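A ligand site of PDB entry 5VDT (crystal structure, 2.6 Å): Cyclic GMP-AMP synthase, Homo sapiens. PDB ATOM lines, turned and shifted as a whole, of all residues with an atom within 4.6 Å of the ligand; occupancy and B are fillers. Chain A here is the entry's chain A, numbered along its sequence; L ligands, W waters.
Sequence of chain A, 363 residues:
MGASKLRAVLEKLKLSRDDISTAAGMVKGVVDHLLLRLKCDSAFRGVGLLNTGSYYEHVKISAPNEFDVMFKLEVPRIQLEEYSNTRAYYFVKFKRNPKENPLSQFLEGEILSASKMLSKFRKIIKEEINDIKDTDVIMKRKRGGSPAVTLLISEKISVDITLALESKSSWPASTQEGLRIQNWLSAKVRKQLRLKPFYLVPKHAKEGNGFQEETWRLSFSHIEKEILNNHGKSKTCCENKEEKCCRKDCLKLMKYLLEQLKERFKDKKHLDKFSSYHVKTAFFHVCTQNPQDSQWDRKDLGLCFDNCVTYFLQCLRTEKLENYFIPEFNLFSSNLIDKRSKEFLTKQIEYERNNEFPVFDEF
The side-chain hydroxyl (OG) of Ser 219 lies within hydrogen-bond range of an oxygen (O1) of the ligand, at 2.6 Å. O6 of the ligand is in salt-bridge range of NZ of Lys 203, 2.7 Å away. An oxygen (O7) of the ligand lies within salt-bridge range of the guanidinium group (NH2) of Arg 217 (2.7 Å). A nitrogen (N1) of the ligand is in hydrogen-bond range of the side-chain hydroxyl (OG) of Ser 221 (2.8 Å). O12 of the ligand sits at hydrogen-bond distance from OG of Ser 275 (3.0 Å). SD of Met 70 sits at hydrogen-bond distance from N2 of the ligand (3.2 Å). The side-chain carboxylate (OD1) of Asp 68 sits at hydrogen-bond distance from a nitrogen (N2) of the ligand, 3.3 Å away.
The side-chain hydroxyl of Ser 219 sits at hydrogen-bond distance from the side-chain hydroxyl of Ser 221, 3.3 Å away. NZ of Lys 203 lies within hydrogen-bond range of O of Gly 145 (2.8 Å). The backbone carbonyl oxygen (O) of Val 201 is in hydrogen-bond range of the backbone NH (N) of Arg 217, at 2.9 Å. The side-chain hydroxyl (OG) of Ser 275 sits close to the backbone NH (N) of Tyr 277. The backbone NH of Ser 275 lies within hydrogen-bond range of a ring nitrogen (ND1) of His 278 (3.2 Å). The side-chain hydroxyl of Tyr 277 sits at hydrogen-bond distance from the side-chain amide nitrogen of Asn 323 (3.2 Å). The side-chain hydroxyl (OH) of Tyr 277 lies close to the side-chain carboxylate (OE2) of Glu 224 (3.3 Å). N of Ala 148 sits close to OG of Ser 146, at 3.3 Å.
O of Gly 145 lies close to O6 of the ligand (3.4 Å). Merely in contact with the ligand: Tyr 277 (3.3 Å), Ala 148 (3.4 Å), Pro 147 (3.5 Å), Thr 162 (3.5 Å), Ser 146 (3.6 Å) and His 278 (3.9 Å). Hydrophobic or aromatic side chains that line the ligand: Met 70, Pro 147, Ala 148 and Tyr 277.
Water W4 bridges O1 of the ligand (2.5 Å) and NE of Arg 217 (3.1 Å). Water W3 lies within hydrogen-bond range of NH1 of Arg 217 (3.0 Å) and O13 of the ligand (3.0 Å). Water W6 lies within hydrogen-bond range of the backbone carbonyl oxygen (O) of Lys 273 (2.9 Å) and an oxygen (O13) of the ligand (3.2 Å). Water W5 lies within hydrogen-bond range of the side-chain hydroxyl of Ser 221 (2.5 Å), the side-chain carboxylate of Glu 224 (3.1 Å) and a nitrogen (N10) of the ligand (3.4 Å).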
ATOM      1  N   ASP A  68      -1.426  13.851 -24.239  1.00  0.00           N
ATOM      2  CA  ASP A  68      -1.154  15.250 -24.576  1.00  0.00           C
ATOM      3  C   ASP A  68      -2.111  15.733 -25.662  1.00  0.00           C
ATOM      4  O   ASP A  68      -1.967  15.396 -26.835  1.00  0.00           O
ATOM      5  CB  ASP A  68       0.290  15.411 -25.045  1.00  0.00           C
ATOM      6  CG  ASP A  68       0.609  16.844 -25.463  1.00  0.00           C
ATOM      7  OD1 ASP A  68       0.426  17.172 -26.653  1.00  0.00           O
ATOM      8  OD2 ASP A  68       1.048  17.629 -24.593  1.00  0.00           O
ATOM      9  N   MET A  70      -4.290  19.177 -27.387  1.00  0.00           N
ATOM     10  CA  MET A  70      -4.091  20.599 -27.617  1.00  0.00           C
ATOM     11  C   MET A  70      -5.401  21.260 -28.009  1.00  0.00           C
ATOM     12  O   MET A  70      -6.076  20.833 -28.943  1.00  0.00           O
ATOM     13  CB  MET A  70      -3.038  20.801 -28.717  1.00  0.00           C
ATOM     14  CG  MET A  70      -2.290  22.120 -28.639  1.00  0.00           C
ATOM     15  SD  MET A  70      -0.859  22.092 -29.736  1.00  0.00           S
ATOM     16  CE  MET A  70      -0.216  23.748 -29.500  1.00  0.00           C
ATOM     17  N   GLY A 145       5.760  28.239 -14.876  1.00  0.00           N
ATOM     18  CA  GLY A 145       5.906  28.736 -16.235  1.00  0.00           C
ATOM     19  C   GLY A 145       5.428  27.781 -17.317  1.00  0.00           C
ATOM     20  O   GLY A 145       5.787  27.932 -18.488  1.00  0.00           O
ATOM     21  N   SER A 146       4.627  26.802 -16.936  1.00  0.00           N
ATOM     22  CA  SER A 146       4.126  25.822 -17.889  1.00  0.00           C
ATOM     23  C   SER A 146       2.757  26.219 -18.428  1.00  0.00           C
ATOM     24  O   SER A 146       1.839  26.508 -17.651  1.00  0.00           O
ATOM     25  CB  SER A 146       4.053  24.431 -17.249  1.00  0.00           C
ATOM     26  OG  SER A 146       3.445  23.497 -18.126  1.00  0.00           O
ATOM     27  N   PRO A 147       2.618  26.257 -19.754  1.00  0.00           N
ATOM     28  CA  PRO A 147       1.359  26.615 -20.411  1.00  0.00           C
ATOM     29  C   PRO A 147       0.325  25.490 -20.354  1.00  0.00           C
ATOM     30  O   PRO A 147      -0.848  25.708 -20.636  1.00  0.00           O
ATOM     31  CB  PRO A 147       1.778  26.892 -21.853  1.00  0.00           C
ATOM     32  CG  PRO A 147       2.949  26.001 -22.062  1.00  0.00           C
ATOM     33  CD  PRO A 147       3.672  25.954 -20.737  1.00  0.00           C
ATOM     34  N   ALA A 148       0.781  24.290 -19.986  1.00  0.00           N
ATOM     35  CA  ALA A 148      -0.099  23.137 -19.953  1.00  0.00           C
ATOM     36  C   ALA A 148      -0.933  23.083 -18.672  1.00  0.00           C
ATOM     37  O   ALA A 148      -0.531  23.557 -17.617  1.00  0.00           O
ATOM     38  CB  ALA A 148       0.719  21.863 -20.079  1.00  0.00           C
ATOM     39  N   ASP A 160      -2.153  16.240 -20.535  1.00  0.00           N
ATOM     40  CA  ASP A 160      -1.722  17.622 -20.624  1.00  0.00           C
ATOM     41  C   ASP A 160      -2.566  18.374 -21.640  1.00  0.00           C
ATOM     42  O   ASP A 160      -2.639  17.974 -22.805  1.00  0.00           O
ATOM     43  CB  ASP A 160      -0.234  17.706 -20.990  1.00  0.00           C
ATOM     44  CG  ASP A 160       0.652  16.984 -19.991  1.00  0.00           C
ATOM     45  OD1 ASP A 160       0.905  15.776 -20.186  1.00  0.00           O
ATOM     46  OD2 ASP A 160       1.110  17.624 -19.021  1.00  0.00           O
ATOM     47  N   THR A 162      -3.088  21.890 -23.537  1.00  0.00           N
ATOM     48  CA  THR A 162      -2.443  23.163 -23.845  1.00  0.00           C
ATOM     49  C   THR A 162      -3.332  24.031 -24.729  1.00  0.00           C
ATOM     50  O   THR A 162      -3.776  23.612 -25.797  1.00  0.00           O
ATOM     51  CB  THR A 162      -1.085  22.950 -24.552  1.00  0.00           C
ATOM     52  OG1 THR A 162      -0.215  22.193 -23.700  1.00  0.00           O
ATOM     53  CG2 THR A 162      -0.438  24.283 -24.873  1.00  0.00           C
ATOM     54  N   VAL A 201       1.179  29.355 -28.014  1.00  0.00           N
ATOM     55  CA  VAL A 201       0.902  28.866 -26.671  1.00  0.00           C
ATOM     56  C   VAL A 201       1.280  29.918 -25.632  1.00  0.00           C
ATOM     57  O   VAL A 201       2.251  30.659 -25.810  1.00  0.00           O
ATOM     58  CB  VAL A 201       1.635  27.529 -26.406  1.00  0.00           C
ATOM     59  CG1 VAL A 201       1.136  26.472 -27.371  1.00  0.00           C
ATOM     60  CG2 VAL A 201       3.138  27.704 -26.534  1.00  0.00           C
ATOM     61  N   LYS A 203       3.187  30.997 -23.297  1.00  0.00           N
ATOM     62  CA  LYS A 203       4.479  30.762 -22.663  1.00  0.00           C
ATOM     63  C   LYS A 203       5.268  32.064 -22.577  1.00  0.00           C
ATOM     64  O   LYS A 203       5.493  32.735 -23.588  1.00  0.00           O
ATOM     65  CB  LYS A 203       5.272  29.706 -23.441  1.00  0.00           C
ATOM     66  CG  LYS A 203       6.693  29.504 -22.951  1.00  0.00           C
ATOM     67  CD  LYS A 203       6.718  28.779 -21.618  1.00  0.00           C
ATOM     68  CE  LYS A 203       8.145  28.559 -21.143  1.00  0.00           C
ATOM     69  NZ  LYS A 203       8.198  27.849 -19.835  1.00  0.00           N
ATOM     70  N   ARG A 217       4.377  31.730 -27.431  1.00  0.00           N
ATOM     71  CA  ARG A 217       5.422  31.048 -28.193  1.00  0.00           C
ATOM     72  C   ARG A 217       4.830  30.331 -29.398  1.00  0.00           C
ATOM     73  O   ARG A 217       3.745  29.745 -29.315  1.00  0.00           O
ATOM     74  CB  ARG A 217       6.190  30.070 -27.302  1.00  0.00           C
ATOM     75  CG  ARG A 217       7.381  29.408 -27.996  1.00  0.00           C
ATOM     76  CD  ARG A 217       8.165  28.535 -27.033  1.00  0.00           C
ATOM     77  NE  ARG A 217       7.378  27.417 -26.508  1.00  0.00           N
ATOM     78  CZ  ARG A 217       7.730  26.694 -25.460  1.00  0.00           C
ATOM     79  NH1 ARG A 217       8.864  26.965 -24.807  1.00  0.00           N
ATOM     80  NH2 ARG A 217       6.957  25.697 -25.038  1.00  0.00           N
ATOM     81  N   SER A 219       4.074  27.576 -32.182  1.00  0.00           N
ATOM     82  CA  SER A 219       3.865  26.141 -32.097  1.00  0.00           C
ATOM     83  C   SER A 219       3.450  25.572 -33.445  1.00  0.00           C
ATOM     84  O   SER A 219       2.545  26.104 -34.109  1.00  0.00           O
ATOM     85  CB  SER A 219       2.823  25.817 -31.028  1.00  0.00           C
ATOM     86  OG  SER A 219       2.697  24.413 -30.856  1.00  0.00           O
ATOM     87  N   SER A 221       3.078  21.928 -33.781  1.00  0.00           N
ATOM     88  CA  SER A 221       2.913  20.528 -33.400  1.00  0.00           C
ATOM     89  C   SER A 221       2.209  19.703 -34.476  1.00  0.00           C
ATOM     90  O   SER A 221       2.529  18.531 -34.704  1.00  0.00           O
ATOM     91  CB  SER A 221       2.148  20.425 -32.081  1.00  0.00           C
ATOM     92  OG  SER A 221       2.789  21.156 -31.054  1.00  0.00           O
ATOM     93  N   GLU A 224       4.531  18.812 -37.113  1.00  0.00           N
ATOM     94  CA  GLU A 224       5.382  17.738 -36.614  1.00  0.00           C
ATOM     95  C   GLU A 224       4.684  16.389 -36.782  1.00  0.00           C
ATOM     96  O   GLU A 224       5.317  15.399 -37.174  1.00  0.00           O
ATOM     97  CB  GLU A 224       5.753  17.972 -35.155  1.00  0.00           C
ATOM     98  CG  GLU A 224       6.540  19.248 -34.916  1.00  0.00           C
ATOM     99  CD  GLU A 224       6.642  19.620 -33.439  1.00  0.00           C
ATOM    100  OE1 GLU A 224       6.428  18.732 -32.587  1.00  0.00           O
ATOM    101  OE2 GLU A 224       6.936  20.790 -33.145  1.00  0.00           O
ATOM    102  N   LYS A 273      14.481  19.310 -17.238  1.00  0.00           N
ATOM    103  CA  LYS A 273      14.230  20.254 -18.324  1.00  0.00           C
ATOM    104  C   LYS A 273      14.291  19.580 -19.699  1.00  0.00           C
ATOM    105  O   LYS A 273      13.819  20.134 -20.686  1.00  0.00           O
ATOM    106  CB  LYS A 273      15.226  21.413 -18.272  1.00  0.00           C
ATOM    107  CG  LYS A 273      15.036  22.334 -17.079  1.00  0.00           C
ATOM    108  CD  LYS A 273      15.925  23.564 -17.177  1.00  0.00           C
ATOM    109  CE  LYS A 273      15.784  24.450 -15.960  1.00  0.00           C
ATOM    110  NZ  LYS A 273      16.637  25.669 -16.060  1.00  0.00           N
ATOM    111  N   SER A 275      13.177  16.987 -22.542  1.00  0.00           N
ATOM    112  CA  SER A 275      11.896  16.393 -22.929  1.00  0.00           C
ATOM    113  C   SER A 275      12.012  15.669 -24.263  1.00  0.00           C
ATOM    114  O   SER A 275      13.004  15.802 -24.970  1.00  0.00           O
ATOM    115  CB  SER A 275      10.806  17.459 -23.000  1.00  0.00           C
ATOM    116  OG  SER A 275      11.038  18.332 -24.089  1.00  0.00           O
ATOM    117  N   TYR A 277      10.619  16.374 -26.862  1.00  0.00           N
ATOM    118  CA  TYR A 277      10.609  17.352 -27.935  1.00  0.00           C
ATOM    119  C   TYR A 277      12.019  17.674 -28.435  1.00  0.00           C
ATOM    120  O   TYR A 277      12.238  17.891 -29.623  1.00  0.00           O
ATOM    121  CB  TYR A 277       9.915  18.652 -27.494  1.00  0.00           C
ATOM    122  CG  TYR A 277       9.795  19.660 -28.606  1.00  0.00           C
ATOM    123  CD1 TYR A 277       8.803  19.554 -29.567  1.00  0.00           C
ATOM    124  CD2 TYR A 277      10.680  20.731 -28.704  1.00  0.00           C
ATOM    125  CE1 TYR A 277       8.684  20.467 -30.588  1.00  0.00           C
ATOM    126  CE2 TYR A 277      10.573  21.660 -29.726  1.00  0.00           C
ATOM    127  CZ  TYR A 277       9.568  21.527 -30.666  1.00  0.00           C
ATOM    128  OH  TYR A 277       9.449  22.440 -31.687  1.00  0.00           O
ATOM    129  N   HIS A 278      12.971  17.708 -27.504  1.00  0.00           N
ATOM    130  CA  HIS A 278      14.375  17.918 -27.862  1.00  0.00           C
ATOM    131  C   HIS A 278      14.847  16.769 -28.744  1.00  0.00           C
ATOM    132  O   HIS A 278      15.452  16.981 -29.806  1.00  0.00           O
ATOM    133  CB  HIS A 278      15.254  18.026 -26.609  1.00  0.00           C
ATOM    134  CG  HIS A 278      14.849  19.140 -25.687  1.00  0.00           C
ATOM    135  ND1 HIS A 278      14.869  19.007 -24.311  1.00  0.00           N
ATOM    136  CD2 HIS A 278      14.435  20.404 -25.932  1.00  0.00           C
ATOM    137  CE1 HIS A 278      14.467  20.134 -23.753  1.00  0.00           C
ATOM    138  NE2 HIS A 278      14.206  21.006 -24.721  1.00  0.00           N
ATOM    139  N   ASN A 323      15.693  25.011 -33.042  1.00  0.00           N
ATOM    140  CA  ASN A 323      14.305  24.678 -33.302  1.00  0.00           C
ATOM    141  C   ASN A 323      14.154  24.403 -34.793  1.00  0.00           C
ATOM    142  O   ASN A 323      14.627  25.175 -35.627  1.00  0.00           O
ATOM    143  CB  ASN A 323      13.376  25.803 -32.854  1.00  0.00           C
ATOM    144  CG  ASN A 323      11.905  25.473 -33.059  1.00  0.00           C
ATOM    145  OD1 ASN A 323      11.406  25.541 -34.180  1.00  0.00           O
ATOM    146  ND2 ASN A 323      11.223  25.119 -31.986  1.00  0.00           N
ATOM    147  N   PHE A 329      16.353  29.913 -32.889  1.00  0.00           N
ATOM    148  CA  PHE A 329      15.876  29.622 -31.537  1.00  0.00           C
ATOM    149  C   PHE A 329      16.586  28.380 -31.003  1.00  0.00           C
ATOM    150  O   PHE A 329      16.334  27.268 -31.477  1.00  0.00           O
ATOM    151  CB  PHE A 329      14.365  29.434 -31.545  1.00  0.00           C
ATOM    152  CG  PHE A 329      13.775  29.178 -30.180  1.00  0.00           C
ATOM    153  CD1 PHE A 329      14.173  29.919 -29.086  1.00  0.00           C
ATOM    154  CD2 PHE A 329      12.814  28.194 -30.008  1.00  0.00           C
ATOM    155  CE1 PHE A 329      13.634  29.682 -27.836  1.00  0.00           C
ATOM    156  CE2 PHE A 329      12.266  27.950 -28.767  1.00  0.00           C
ATOM    157  CZ  PHE A 329      12.677  28.693 -27.676  1.00  0.00           C
ATOM    158  N   LEU A 331      17.251  25.588 -28.375  1.00  0.00           N
ATOM    159  CA  LEU A 331      16.593  24.867 -27.296  1.00  0.00           C
ATOM    160  C   LEU A 331      17.582  24.447 -26.220  1.00  0.00           C
ATOM    161  O   LEU A 331      17.191  24.155 -25.091  1.00  0.00           O
ATOM    162  CB  LEU A 331      15.870  23.639 -27.849  1.00  0.00           C
ATOM    163  CG  LEU A 331      14.843  23.899 -28.948  1.00  0.00           C
ATOM    164  CD1 LEU A 331      14.285  22.598 -29.503  1.00  0.00           C
ATOM    165  CD2 LEU A 331      13.720  24.787 -28.429  1.00  0.00           C
HETATM  166  O1  LIG L   1       3.972  23.873 -28.630  1.00  0.00           O
HETATM  167  C1  LIG L   1       3.461  23.099 -27.891  1.00  0.00           C
HETATM  168  N1  LIG L   1       2.564  22.102 -28.396  1.00  0.00           N
HETATM  169  C2  LIG L   1       1.944  21.169 -27.483  1.00  0.00           C
HETATM  170  N2  LIG L   1       1.017  20.119 -27.997  1.00  0.00           N
HETATM  171  N3  LIG L   1       2.241  21.233 -26.049  1.00  0.00           N
HETATM  172  C3  LIG L   1       3.177  22.277 -25.537  1.00  0.00           C
HETATM  173  C4  LIG L   1       3.764  23.174 -26.394  1.00  0.00           C
HETATM  174  N4  LIG L   1       4.566  24.019 -25.656  1.00  0.00           N
HETATM  175  C5  LIG L   1       4.480  23.647 -24.358  1.00  0.00           C
HETATM  176  N5  LIG L   1       3.613  22.562 -24.288  1.00  0.00           N
HETATM  177  C6  LIG L   1       3.228  21.837 -23.032  1.00  0.00           C
HETATM  178  C7  LIG L   1       3.980  20.416 -23.108  1.00  0.00           C
HETATM  179  O2  LIG L   1       3.108  19.352 -22.533  1.00  0.00           O
HETATM  180  O3  LIG L   1       3.665  22.451 -21.716  1.00  0.00           O
HETATM  181  C8  LIG L   1       4.518  21.601 -21.175  1.00  0.00           C
HETATM  182  C9  LIG L   1       5.709  22.321 -20.620  1.00  0.00           C
HETATM  183  O4  LIG L   1       6.011  23.430 -21.476  1.00  0.00           O
HETATM  184  P1  LIG L   1       7.406  24.307 -21.184  1.00  0.00           P
HETATM  185  O5  LIG L   1       8.768  23.364 -21.127  1.00  0.00           O
HETATM  186  O6  LIG L   1       7.301  25.288 -20.026  1.00  0.00           O
HETATM  187  O7  LIG L   1       7.561  25.180 -22.409  1.00  0.00           O
HETATM  188  C10 LIG L   1       4.993  20.591 -22.405  1.00  0.00           C
HETATM  189  O8  LIG L   1       5.449  19.327 -21.837  1.00  0.00           O
HETATM  190  P2  LIG L   1       6.975  18.740 -22.348  1.00  0.00           P
HETATM  191  O9  LIG L   1       7.474  17.557 -21.550  1.00  0.00           O
HETATM  192  O10 LIG L   1       6.699  18.191 -23.720  1.00  0.00           O
HETATM  193  O11 LIG L   1       8.174  19.955 -22.604  1.00  0.00           O
HETATM  194  C11 LIG L   1       8.988  20.350 -21.513  1.00  0.00           C
HETATM  195  C12 LIG L   1       9.822  21.560 -21.996  1.00  0.00           C
HETATM  196  O12 LIG L   1      10.553  21.211 -23.400  1.00  0.00           O
HETATM  197  C13 LIG L   1       9.053  22.537 -22.291  1.00  0.00           C
HETATM  198  C14 LIG L   1       9.913  23.391 -23.415  1.00  0.00           C
HETATM  199  O13 LIG L   1      11.020  24.066 -22.781  1.00  0.00           O
HETATM  200  C15 LIG L   1      10.360  22.449 -24.262  1.00  0.00           C
HETATM  201  N6  LIG L   1       9.392  22.256 -25.335  1.00  0.00           N
HETATM  202  C16 LIG L   1       8.516  21.268 -25.416  1.00  0.00           C
HETATM  203  N7  LIG L   1       7.791  21.440 -26.546  1.00  0.00           N
HETATM  204  C17 LIG L   1       8.220  22.568 -27.171  1.00  0.00           C
HETATM  205  C18 LIG L   1       9.216  23.095 -26.425  1.00  0.00           C
HETATM  206  N8  LIG L   1       9.832  24.246 -26.846  1.00  0.00           N
HETATM  207  C19 LIG L   1       9.453  24.859 -27.986  1.00  0.00           C
HETATM  208  N9  LIG L   1       8.481  24.377 -28.723  1.00  0.00           N
HETATM  209  C20 LIG L   1       7.837  23.242 -28.375  1.00  0.00           C
HETATM  210  N10 LIG L   1       6.744  22.707 -29.222  1.00  0.00           N
HETATM  211  O   HOH W   1      12.279  25.280 -25.257  1.00  0.00           O
HETATM  212  O   HOH W   2       5.598  19.538 -27.405  1.00  0.00           O
HETATM  213  O   HOH W   3      10.769  27.059 -22.505  1.00  0.00           O
HETATM  214  O   HOH W   4       5.346  25.975 -28.328  1.00  0.00           O
HETATM  215  O   HOH W   5       4.881  20.063 -30.283  1.00  0.00           O
HETATM  216  O   HOH W   6      13.534  22.943 -21.209  1.00  0.00           O
